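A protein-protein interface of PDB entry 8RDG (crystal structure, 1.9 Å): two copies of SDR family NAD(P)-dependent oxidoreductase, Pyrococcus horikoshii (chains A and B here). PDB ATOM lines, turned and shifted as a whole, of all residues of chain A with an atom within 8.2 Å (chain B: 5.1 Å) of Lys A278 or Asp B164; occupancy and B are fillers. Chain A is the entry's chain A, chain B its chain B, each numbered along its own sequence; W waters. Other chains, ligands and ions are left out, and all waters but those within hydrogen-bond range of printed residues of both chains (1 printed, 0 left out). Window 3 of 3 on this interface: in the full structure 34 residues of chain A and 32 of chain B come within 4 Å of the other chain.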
ATOM      1  N   VAL A  82     -13.488   9.954  -0.214  1.00  0.00           N
ATOM      2  CA  VAL A  82     -13.498  11.396   0.020  1.00  0.00           C
ATOM      3  C   VAL A  82     -14.258  11.736   1.296  1.00  0.00           C
ATOM      4  O   VAL A  82     -13.866  12.647   2.036  1.00  0.00           O
ATOM      5  CB  VAL A  82     -14.107  12.149  -1.182  1.00  0.00           C
ATOM      6  CG1 VAL A  82     -13.869  13.644  -1.040  1.00  0.00           C
ATOM      7  CG2 VAL A  82     -13.550  11.653  -2.501  1.00  0.00           C
ATOM      8  N   ARG A  83     -15.331  10.992   1.593  1.00  0.00           N
ATOM      9  CA  ARG A  83     -16.220  11.346   2.704  1.00  0.00           C
ATOM     10  C   ARG A  83     -15.509  11.405   4.039  1.00  0.00           C
ATOM     11  O   ARG A  83     -15.956  12.126   4.935  1.00  0.00           O
ATOM     12  CB  ARG A  83     -17.364  10.338   2.831  1.00  0.00           C
ATOM     13  CG  ARG A  83     -18.215  10.186   1.613  1.00  0.00           C
ATOM     14  CD  ARG A  83     -19.252   9.101   1.828  1.00  0.00           C
ATOM     15  NE  ARG A  83     -19.940   8.787   0.582  1.00  0.00           N
ATOM     16  CZ  ARG A  83     -20.998   7.993   0.490  1.00  0.00           C
ATOM     17  NH1 ARG A  83     -21.516   7.408   1.562  1.00  0.00           N
ATOM     18  NH2 ARG A  83     -21.549   7.778  -0.707  1.00  0.00           N
ATOM     19  N   ILE A  84     -14.466  10.588   4.227  1.00  0.00           N
ATOM     20  CA  ILE A  84     -13.796  10.469   5.523  1.00  0.00           C
ATOM     21  C   ILE A  84     -12.862  11.631   5.802  1.00  0.00           C
ATOM     22  O   ILE A  84     -12.194  11.643   6.847  1.00  0.00           O
ATOM     23  CB  ILE A  84     -13.077   9.106   5.628  1.00  0.00           C
ATOM     24  CG1 ILE A  84     -11.780   9.069   4.822  1.00  0.00           C
ATOM     25  CG2 ILE A  84     -14.005   7.990   5.149  1.00  0.00           C
ATOM     26  CD1 ILE A  84     -10.965   7.778   5.045  1.00  0.00           C
ATOM     27  N   GLY A  85     -12.783  12.599   4.884  1.00  0.00           N
ATOM     28  CA  GLY A  85     -11.803  13.664   5.016  1.00  0.00           C
ATOM     29  C   GLY A  85     -11.966  14.521   6.255  1.00  0.00           C
ATOM     30  O   GLY A  85     -10.974  14.953   6.846  1.00  0.00           O
ATOM     31  N   SER A  86     -13.201  14.783   6.678  1.00  0.00           N
ATOM     32  CA  SER A  86     -13.283  15.685   7.818  1.00  0.00           C
ATOM     33  C   SER A  86     -13.210  14.961   9.154  1.00  0.00           C
ATOM     34  O   SER A  86     -13.005  15.615  10.181  1.00  0.00           O
ATOM     35  CB  SER A  86     -14.560  16.539   7.746  1.00  0.00           C
ATOM     36  OG  SER A  86     -15.686  15.761   7.420  1.00  0.00           O
ATOM     37  N   GLN A  87     -13.301  13.632   9.171  1.00  0.00           N
ATOM     38  CA  GLN A  87     -13.077  12.863  10.395  1.00  0.00           C
ATOM     39  C   GLN A  87     -11.687  12.246  10.478  1.00  0.00           C
ATOM     40  O   GLN A  87     -11.096  12.201  11.560  1.00  0.00           O
ATOM     41  CB  GLN A  87     -14.137  11.769  10.554  1.00  0.00           C
ATOM     42  CG  GLN A  87     -15.535  12.334  10.796  1.00  0.00           C
ATOM     43  CD  GLN A  87     -16.577  11.255  11.048  1.00  0.00           C
ATOM     44  OE1 GLN A  87     -16.248  10.074  11.185  1.00  0.00           O
ATOM     45  NE2 GLN A  87     -17.842  11.663  11.131  1.00  0.00           N
ATOM     46  N   ILE A 142     -10.737  20.961  -2.858  1.00  0.00           N
ATOM     47  CA  ILE A 142     -11.588  21.334  -1.732  1.00  0.00           C
ATOM     48  C   ILE A 142     -11.728  20.216  -0.723  1.00  0.00           C
ATOM     49  O   ILE A 142     -12.419  20.396   0.281  1.00  0.00           O
ATOM     50  CB  ILE A 142     -12.985  21.796  -2.193  1.00  0.00           C
ATOM     51  CG1 ILE A 142     -13.787  20.631  -2.796  1.00  0.00           C
ATOM     52  CG2 ILE A 142     -12.873  22.932  -3.182  1.00  0.00           C
ATOM     53  CD1 ILE A 142     -15.257  21.015  -3.067  1.00  0.00           C
ATOM     54  N   SER A 143     -11.106  19.065  -0.956  1.00  0.00           N
ATOM     55  CA  SER A 143     -11.153  17.987   0.011  1.00  0.00           C
ATOM     56  C   SER A 143      -9.736  17.586   0.387  1.00  0.00           C
ATOM     57  O   SER A 143      -8.776  17.804  -0.364  1.00  0.00           O
ATOM     58  CB  SER A 143     -11.910  16.772  -0.534  1.00  0.00           C
ATOM     59  OG  SER A 143     -11.273  16.251  -1.704  1.00  0.00           O
ATOM     60  N   VAL A 144      -9.620  16.969   1.561  1.00  0.00           N
ATOM     61  CA  VAL A 144      -8.327  16.413   1.943  1.00  0.00           C
ATOM     62  C   VAL A 144      -7.899  15.347   0.948  1.00  0.00           C
ATOM     63  O   VAL A 144      -6.710  15.224   0.638  1.00  0.00           O
ATOM     64  CB  VAL A 144      -8.381  15.861   3.382  1.00  0.00           C
ATOM     65  CG1 VAL A 144      -7.105  15.083   3.704  1.00  0.00           C
ATOM     66  CG2 VAL A 144      -8.545  17.020   4.376  1.00  0.00           C
ATOM     67  N   TYR A 145      -8.853  14.583   0.407  1.00  0.00           N
ATOM     68  CA  TYR A 145      -8.503  13.546  -0.562  1.00  0.00           C
ATOM     69  C   TYR A 145      -7.953  14.152  -1.850  1.00  0.00           C
ATOM     70  O   TYR A 145      -6.908  13.715  -2.358  1.00  0.00           O
ATOM     71  CB  TYR A 145      -9.725  12.682  -0.861  1.00  0.00           C
ATOM     72  CG  TYR A 145      -9.551  11.748  -2.050  1.00  0.00           C
ATOM     73  CD1 TYR A 145      -8.815  10.570  -1.929  1.00  0.00           C
ATOM     74  CD2 TYR A 145     -10.151  12.022  -3.276  1.00  0.00           C
ATOM     75  CE1 TYR A 145      -8.664   9.709  -2.993  1.00  0.00           C
ATOM     76  CE2 TYR A 145     -10.016  11.160  -4.347  1.00  0.00           C
ATOM     77  CZ  TYR A 145      -9.269   9.995  -4.199  1.00  0.00           C
ATOM     78  OH  TYR A 145      -9.116   9.123  -5.260  1.00  0.00           O
ATOM     79  N   GLY A 270     -27.534  18.232   3.020  1.00  0.00           N
ATOM     80  CA  GLY A 270     -26.104  18.371   2.828  1.00  0.00           C
ATOM     81  C   GLY A 270     -25.454  19.507   3.603  1.00  0.00           C
ATOM     82  O   GLY A 270     -25.909  19.916   4.676  1.00  0.00           O
ATOM     83  N   VAL A 271     -24.358  20.023   3.035  1.00  0.00           N
ATOM     84  CA  VAL A 271     -23.582  21.107   3.632  1.00  0.00           C
ATOM     85  C   VAL A 271     -23.023  21.969   2.511  1.00  0.00           C
ATOM     86  O   VAL A 271     -22.895  21.530   1.364  1.00  0.00           O
ATOM     87  CB  VAL A 271     -22.414  20.606   4.524  1.00  0.00           C
ATOM     88  CG1 VAL A 271     -22.917  20.057   5.846  1.00  0.00           C
ATOM     89  CG2 VAL A 271     -21.587  19.559   3.785  1.00  0.00           C
ATOM     90  N   ASP A 272     -22.662  23.202   2.864  1.00  0.00           N
ATOM     91  CA  ASP A 272     -22.023  24.132   1.938  1.00  0.00           C
ATOM     92  C   ASP A 272     -22.804  24.236   0.629  1.00  0.00           C
ATOM     93  O   ASP A 272     -22.231  24.328  -0.458  1.00  0.00           O
ATOM     94  CB  ASP A 272     -20.575  23.712   1.670  1.00  0.00           C
ATOM     95  CG  ASP A 272     -19.702  23.779   2.913  1.00  0.00           C
ATOM     96  OD1 ASP A 272     -19.923  24.660   3.773  1.00  0.00           O
ATOM     97  OD2 ASP A 272     -18.789  22.939   3.030  1.00  0.00           O
ATOM     98  N   ARG A 275     -23.988  19.932  -0.855  1.00  0.00           N
ATOM     99  CA  ARG A 275     -22.988  18.877  -0.990  1.00  0.00           C
ATOM    100  C   ARG A 275     -23.271  17.741  -0.010  1.00  0.00           C
ATOM    101  O   ARG A 275     -23.796  17.955   1.080  1.00  0.00           O
ATOM    102  CB  ARG A 275     -21.583  19.427  -0.722  1.00  0.00           C
ATOM    103  CG  ARG A 275     -21.226  20.674  -1.481  1.00  0.00           C
ATOM    104  CD  ARG A 275     -19.892  21.208  -1.003  1.00  0.00           C
ATOM    105  NE  ARG A 275     -19.599  22.498  -1.609  1.00  0.00           N
ATOM    106  CZ  ARG A 275     -18.940  22.671  -2.749  1.00  0.00           C
ATOM    107  NH1 ARG A 275     -18.446  21.645  -3.428  1.00  0.00           N
ATOM    108  NH2 ARG A 275     -18.764  23.906  -3.214  1.00  0.00           N
ATOM    109  N   GLY A 276     -22.894  16.522  -0.393  1.00  0.00           N
ATOM    110  CA  GLY A 276     -23.155  15.382   0.471  1.00  0.00           C
ATOM    111  C   GLY A 276     -22.316  15.373   1.729  1.00  0.00           C
ATOM    112  O   GLY A 276     -22.734  14.835   2.758  1.00  0.00           O
ATOM    113  N   TRP A 277     -21.129  15.956   1.667  1.00  0.00           N
ATOM    114  CA  TRP A 277     -20.212  16.021   2.796  1.00  0.00           C
ATOM    115  C   TRP A 277     -19.277  17.185   2.535  1.00  0.00           C
ATOM    116  O   TRP A 277     -19.246  17.732   1.432  1.00  0.00           O
ATOM    117  CB  TRP A 277     -19.435  14.714   2.966  1.00  0.00           C
ATOM    118  CG  TRP A 277     -18.939  14.163   1.657  1.00  0.00           C
ATOM    119  CD1 TRP A 277     -17.746  14.440   1.030  1.00  0.00           C
ATOM    120  CD2 TRP A 277     -19.634  13.240   0.804  1.00  0.00           C
ATOM    121  NE1 TRP A 277     -17.663  13.737  -0.161  1.00  0.00           N
ATOM    122  CE2 TRP A 277     -18.810  12.997  -0.318  1.00  0.00           C
ATOM    123  CE3 TRP A 277     -20.874  12.587   0.888  1.00  0.00           C
ATOM    124  CZ2 TRP A 277     -19.190  12.132  -1.350  1.00  0.00           C
ATOM    125  CZ3 TRP A 277     -21.253  11.733  -0.144  1.00  0.00           C
ATOM    126  CH2 TRP A 277     -20.415  11.514  -1.247  1.00  0.00           C
ATOM    127  N   LYS A 278     -18.533  17.570   3.572  1.00  0.00           N
ATOM    128  CA  LYS A 278     -17.452  18.532   3.411  1.00  0.00           C
ATOM    129  C   LYS A 278     -16.515  18.092   2.294  1.00  0.00           C
ATOM    130  O   LYS A 278     -16.038  16.955   2.285  1.00  0.00           O
ATOM    131  CB  LYS A 278     -16.660  18.663   4.719  1.00  0.00           C
ATOM    132  CG  LYS A 278     -17.203  19.696   5.689  1.00  0.00           C
ATOM    133  CD  LYS A 278     -17.210  21.087   5.076  1.00  0.00           C
ATOM    134  CE  LYS A 278     -17.116  22.137   6.167  1.00  0.00           C
ATOM    135  NZ  LYS A 278     -17.415  23.499   5.662  1.00  0.00           N
ATOM    136  N   GLY A 279     -16.279  18.982   1.329  1.00  0.00           N
ATOM    137  CA  GLY A 279     -15.322  18.674   0.285  1.00  0.00           C
ATOM    138  C   GLY A 279     -15.890  17.961  -0.922  1.00  0.00           C
ATOM    139  O   GLY A 279     -15.131  17.633  -1.841  1.00  0.00           O
ATOM    140  N   ASP A 280     -17.194  17.712  -0.949  1.00  0.00           N
ATOM    141  CA  ASP A 280     -17.823  17.027  -2.060  1.00  0.00           C
ATOM    142  C   ASP A 280     -18.000  18.004  -3.217  1.00  0.00           C
ATOM    143  O   ASP A 280     -18.736  18.990  -3.101  1.00  0.00           O
ATOM    144  CB  ASP A 280     -19.163  16.454  -1.594  1.00  0.00           C
ATOM    145  CG  ASP A 280     -19.878  15.674  -2.676  1.00  0.00           C
ATOM    146  OD1 ASP A 280     -19.176  15.065  -3.511  1.00  0.00           O
ATOM    147  OD2 ASP A 280     -21.135  15.664  -2.678  1.00  0.00           O
ATOM    148  N   VAL A 281     -17.333  17.728  -4.336  1.00  0.00           N
ATOM    149  CA  VAL A 281     -17.448  18.584  -5.518  1.00  0.00           C
ATOM    150  C   VAL A 281     -18.862  18.519  -6.091  1.00  0.00           C
ATOM    151  O   VAL A 281     -19.454  17.437  -6.206  1.00  0.00           O
ATOM    152  CB  VAL A 281     -16.391  18.166  -6.560  1.00  0.00           C
ATOM    153  CG1 VAL A 281     -16.674  18.811  -7.904  1.00  0.00           C
ATOM    154  CG2 VAL A 281     -14.972  18.533  -6.041  1.00  0.00           C
ATOM    155  N   TYR B 159      -7.238  21.435   3.264  1.00  0.00           N
ATOM    156  CA  TYR B 159      -7.581  21.650   4.667  1.00  0.00           C
ATOM    157  C   TYR B 159      -8.381  22.922   4.840  1.00  0.00           C
ATOM    158  O   TYR B 159      -9.294  22.980   5.672  1.00  0.00           O
ATOM    159  CB  TYR B 159      -6.326  21.724   5.527  1.00  0.00           C
ATOM    160  CG  TYR B 159      -5.839  20.388   6.020  1.00  0.00           C
ATOM    161  CD1 TYR B 159      -5.271  19.455   5.159  1.00  0.00           C
ATOM    162  CD2 TYR B 159      -5.932  20.069   7.368  1.00  0.00           C
ATOM    163  CE1 TYR B 159      -4.814  18.215   5.641  1.00  0.00           C
ATOM    164  CE2 TYR B 159      -5.477  18.862   7.853  1.00  0.00           C
ATOM    165  CZ  TYR B 159      -4.929  17.942   7.001  1.00  0.00           C
ATOM    166  OH  TYR B 159      -4.505  16.762   7.568  1.00  0.00           O
ATOM    167  N   ALA B 160      -8.024  23.967   4.093  1.00  0.00           N
ATOM    168  CA  ALA B 160      -8.741  25.225   4.208  1.00  0.00           C
ATOM    169  C   ALA B 160     -10.214  25.013   3.908  1.00  0.00           C
ATOM    170  O   ALA B 160     -11.086  25.440   4.675  1.00  0.00           O
ATOM    171  CB  ALA B 160      -8.117  26.265   3.276  1.00  0.00           C
ATOM    172  N   HIS B 161     -10.506  24.304   2.815  1.00  0.00           N
ATOM    173  CA  HIS B 161     -11.905  24.064   2.457  1.00  0.00           C
ATOM    174  C   HIS B 161     -12.590  23.114   3.432  1.00  0.00           C
ATOM    175  O   HIS B 161     -13.783  23.274   3.726  1.00  0.00           O
ATOM    176  CB  HIS B 161     -12.001  23.520   1.030  1.00  0.00           C
ATOM    177  CG  HIS B 161     -11.865  24.579  -0.016  1.00  0.00           C
ATOM    178  ND1 HIS B 161     -12.920  25.369  -0.418  1.00  0.00           N
ATOM    179  CD2 HIS B 161     -10.793  24.982  -0.742  1.00  0.00           C
ATOM    180  CE1 HIS B 161     -12.508  26.211  -1.350  1.00  0.00           C
ATOM    181  NE2 HIS B 161     -11.221  25.996  -1.567  1.00  0.00           N
ATOM    182  N   THR B 162     -11.865  22.110   3.937  1.00  0.00           N
ATOM    183  CA  THR B 162     -12.513  21.082   4.752  1.00  0.00           C
ATOM    184  C   THR B 162     -12.757  21.540   6.184  1.00  0.00           C
ATOM    185  O   THR B 162     -13.766  21.164   6.790  1.00  0.00           O
ATOM    186  CB  THR B 162     -11.667  19.799   4.752  1.00  0.00           C
ATOM    187  OG1 THR B 162     -11.593  19.258   3.425  1.00  0.00           O
ATOM    188  CG2 THR B 162     -12.248  18.740   5.703  1.00  0.00           C
ATOM    189  N   PHE B 163     -11.860  22.350   6.736  1.00  0.00           N
ATOM    190  CA  PHE B 163     -11.906  22.737   8.138  1.00  0.00           C
ATOM    191  C   PHE B 163     -12.115  24.234   8.317  1.00  0.00           C
ATOM    192  O   PHE B 163     -11.822  24.763   9.389  1.00  0.00           O
ATOM    193  CB  PHE B 163     -10.637  22.272   8.854  1.00  0.00           C
ATOM    194  CG  PHE B 163     -10.449  20.792   8.812  1.00  0.00           C
ATOM    195  CD1 PHE B 163     -11.271  19.960   9.564  1.00  0.00           C
ATOM    196  CD2 PHE B 163      -9.491  20.222   7.980  1.00  0.00           C
ATOM    197  CE1 PHE B 163     -11.124  18.576   9.512  1.00  0.00           C
ATOM    198  CE2 PHE B 163      -9.338  18.841   7.922  1.00  0.00           C
ATOM    199  CZ  PHE B 163     -10.155  18.014   8.689  1.00  0.00           C
ATOM    200  N   ASP B 164     -12.592  24.926   7.279  1.00  0.00           N
ATOM    201  CA  ASP B 164     -13.156  26.276   7.385  1.00  0.00           C
ATOM    202  C   ASP B 164     -12.164  27.288   7.961  1.00  0.00           C
ATOM    203  O   ASP B 164     -12.403  27.917   8.993  1.00  0.00           O
ATOM    204  CB  ASP B 164     -14.436  26.266   8.237  1.00  0.00           C
ATOM    205  CG  ASP B 164     -15.620  25.643   7.531  1.00  0.00           C
ATOM    206  OD1 ASP B 164     -15.512  25.323   6.324  1.00  0.00           O
ATOM    207  OD2 ASP B 164     -16.672  25.471   8.190  1.00  0.00           O
ATOM    208  N   PHE B 165     -11.049  27.458   7.267  1.00  0.00           N
ATOM    209  CA  PHE B 165     -10.217  28.636   7.458  1.00  0.00           C
ATOM    210  C   PHE B 165      -9.817  29.120   6.076  1.00  0.00           C
ATOM    211  O   PHE B 165     -10.096  28.464   5.073  1.00  0.00           O
ATOM    212  CB  PHE B 165      -9.000  28.347   8.353  1.00  0.00           C
ATOM    213  CG  PHE B 165      -8.068  27.317   7.788  1.00  0.00           C
ATOM    214  CD1 PHE B 165      -7.059  27.691   6.919  1.00  0.00           C
ATOM    215  CD2 PHE B 165      -8.204  25.970   8.127  1.00  0.00           C
ATOM    216  CE1 PHE B 165      -6.208  26.750   6.386  1.00  0.00           C
ATOM    217  CE2 PHE B 165      -7.346  25.025   7.600  1.00  0.00           C
ATOM    218  CZ  PHE B 165      -6.341  25.420   6.734  1.00  0.00           C
ATOM    219  N   ARG B 166      -9.153  30.268   6.009  1.00  0.00           N
ATOM    220  CA  ARG B 166      -8.832  30.874   4.726  1.00  0.00           C
ATOM    221  C   ARG B 166      -7.325  30.901   4.526  1.00  0.00           C
ATOM    222  O   ARG B 166      -6.577  31.131   5.478  1.00  0.00           O
ATOM    223  CB  ARG B 166      -9.416  32.284   4.643  1.00  0.00           C
ATOM    224  CG  ARG B 166     -10.941  32.298   4.727  1.00  0.00           C
ATOM    225  CD  ARG B 166     -11.473  33.723   4.673  1.00  0.00           C
ATOM    226  NE  ARG B 166     -11.118  34.331   3.402  1.00  0.00           N
ATOM    227  CZ  ARG B 166     -10.774  35.602   3.246  1.00  0.00           C
ATOM    228  NH1 ARG B 166     -10.761  36.447   4.264  1.00  0.00           N
ATOM    229  NH2 ARG B 166     -10.432  36.035   2.036  1.00  0.00           N
ATOM    230  N   ARG B 234     -11.803  31.851  -0.311  1.00  0.00           N
ATOM    231  CA  ARG B 234     -11.345  30.876   0.670  1.00  0.00           C
ATOM    232  C   ARG B 234      -9.848  30.606   0.508  1.00  0.00           C
ATOM    233  O   ARG B 234      -9.086  30.623   1.483  1.00  0.00           O
ATOM    234  CB  ARG B 234     -12.166  29.599   0.523  1.00  0.00           C
ATOM    235  CG  ARG B 234     -11.555  28.397   1.212  1.00  0.00           C
ATOM    236  CD  ARG B 234     -11.994  28.343   2.638  1.00  0.00           C
ATOM    237  NE  ARG B 234     -13.423  28.084   2.740  1.00  0.00           N
ATOM    238  CZ  ARG B 234     -14.154  28.374   3.806  1.00  0.00           C
ATOM    239  NH1 ARG B 234     -13.616  28.928   4.883  1.00  0.00           N
ATOM    240  NH2 ARG B 234     -15.453  28.090   3.797  1.00  0.00           N
HETATM  241  O   HOH W   1     -12.279  16.666   2.965  1.00  0.00           O
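Phe B163 touches Gly A85. CB of Ser A86 touches CG2 of Thr B162, 3.8 Å away. Phe B163 touches Ser A86 (CE1 to O, 3.6 Å). Ile A142 touches His B161 (O to CB, 3.2 Å). CA of Ser A143 touches OG1 of Thr B162, 3.7 Å away. N of Val A144 touches OG1 of Thr B162 (3.6 Å). Lys A278 touches Thr B162.
The side-chain hydroxyl of Thr B162 lies within hydrogen-bond range of the backbone carbonyl oxygen of Ile A142. The side-chain amino group (NZ) of Lys A278 is in salt-bridge range of the side-chain carboxylate (OD1) of Asp B164 (2.7 Å).
Of the 20 printed residues of chain A, 6 touch a printed residue of chain B. Printed residues of chain A that touch a printed residue of chain B: Gly A85, Ser A86, Ile A142, Ser A143, Val A144 and Lys A278. Hydrophobic or aromatic side chains of chain A that line the printed part of chain B: Ile A142 and Val A144. Of the 9 printed residues of chain B, 4 touch a printed residue of chain A.
No position is printed for both chains. Of the 9 pairs that touch across the chains among the printed residues, none has its exchanged pair printed and touching as well.
Water W1 lies within hydrogen-bond range of OG1 of Thr B162 (2.7 Å) and N of Val A144 (3.0 Å).
Of chain A, only Lys A278 comes within 4 Å of Asp B164. Of the printed residues of chain A, Thr B162 touches Ser A86, Ile A142, Ser A143, Val A144 and Lys A278. Printed residues of chain A within 4 Å of His B161: Ile A142. Printed residues of chain B within 4 Å of Ser A143: Thr B162. Printed residues of chain A within 4 Å of Phe B163: Gly A85 (3.7 Å) and Ser A86 (3.6 Å). Asp A272 touches none of the printed residues of chain B.
The side-chain carboxylate (OD2) of Asp A272 lies within salt-bridge range of the side-chain amino group (NZ) of Lys A278 (3.0 Å). OD1 of Asp B164 lies within salt-bridge range of NH2 of Arg B234 (3.7 Å).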
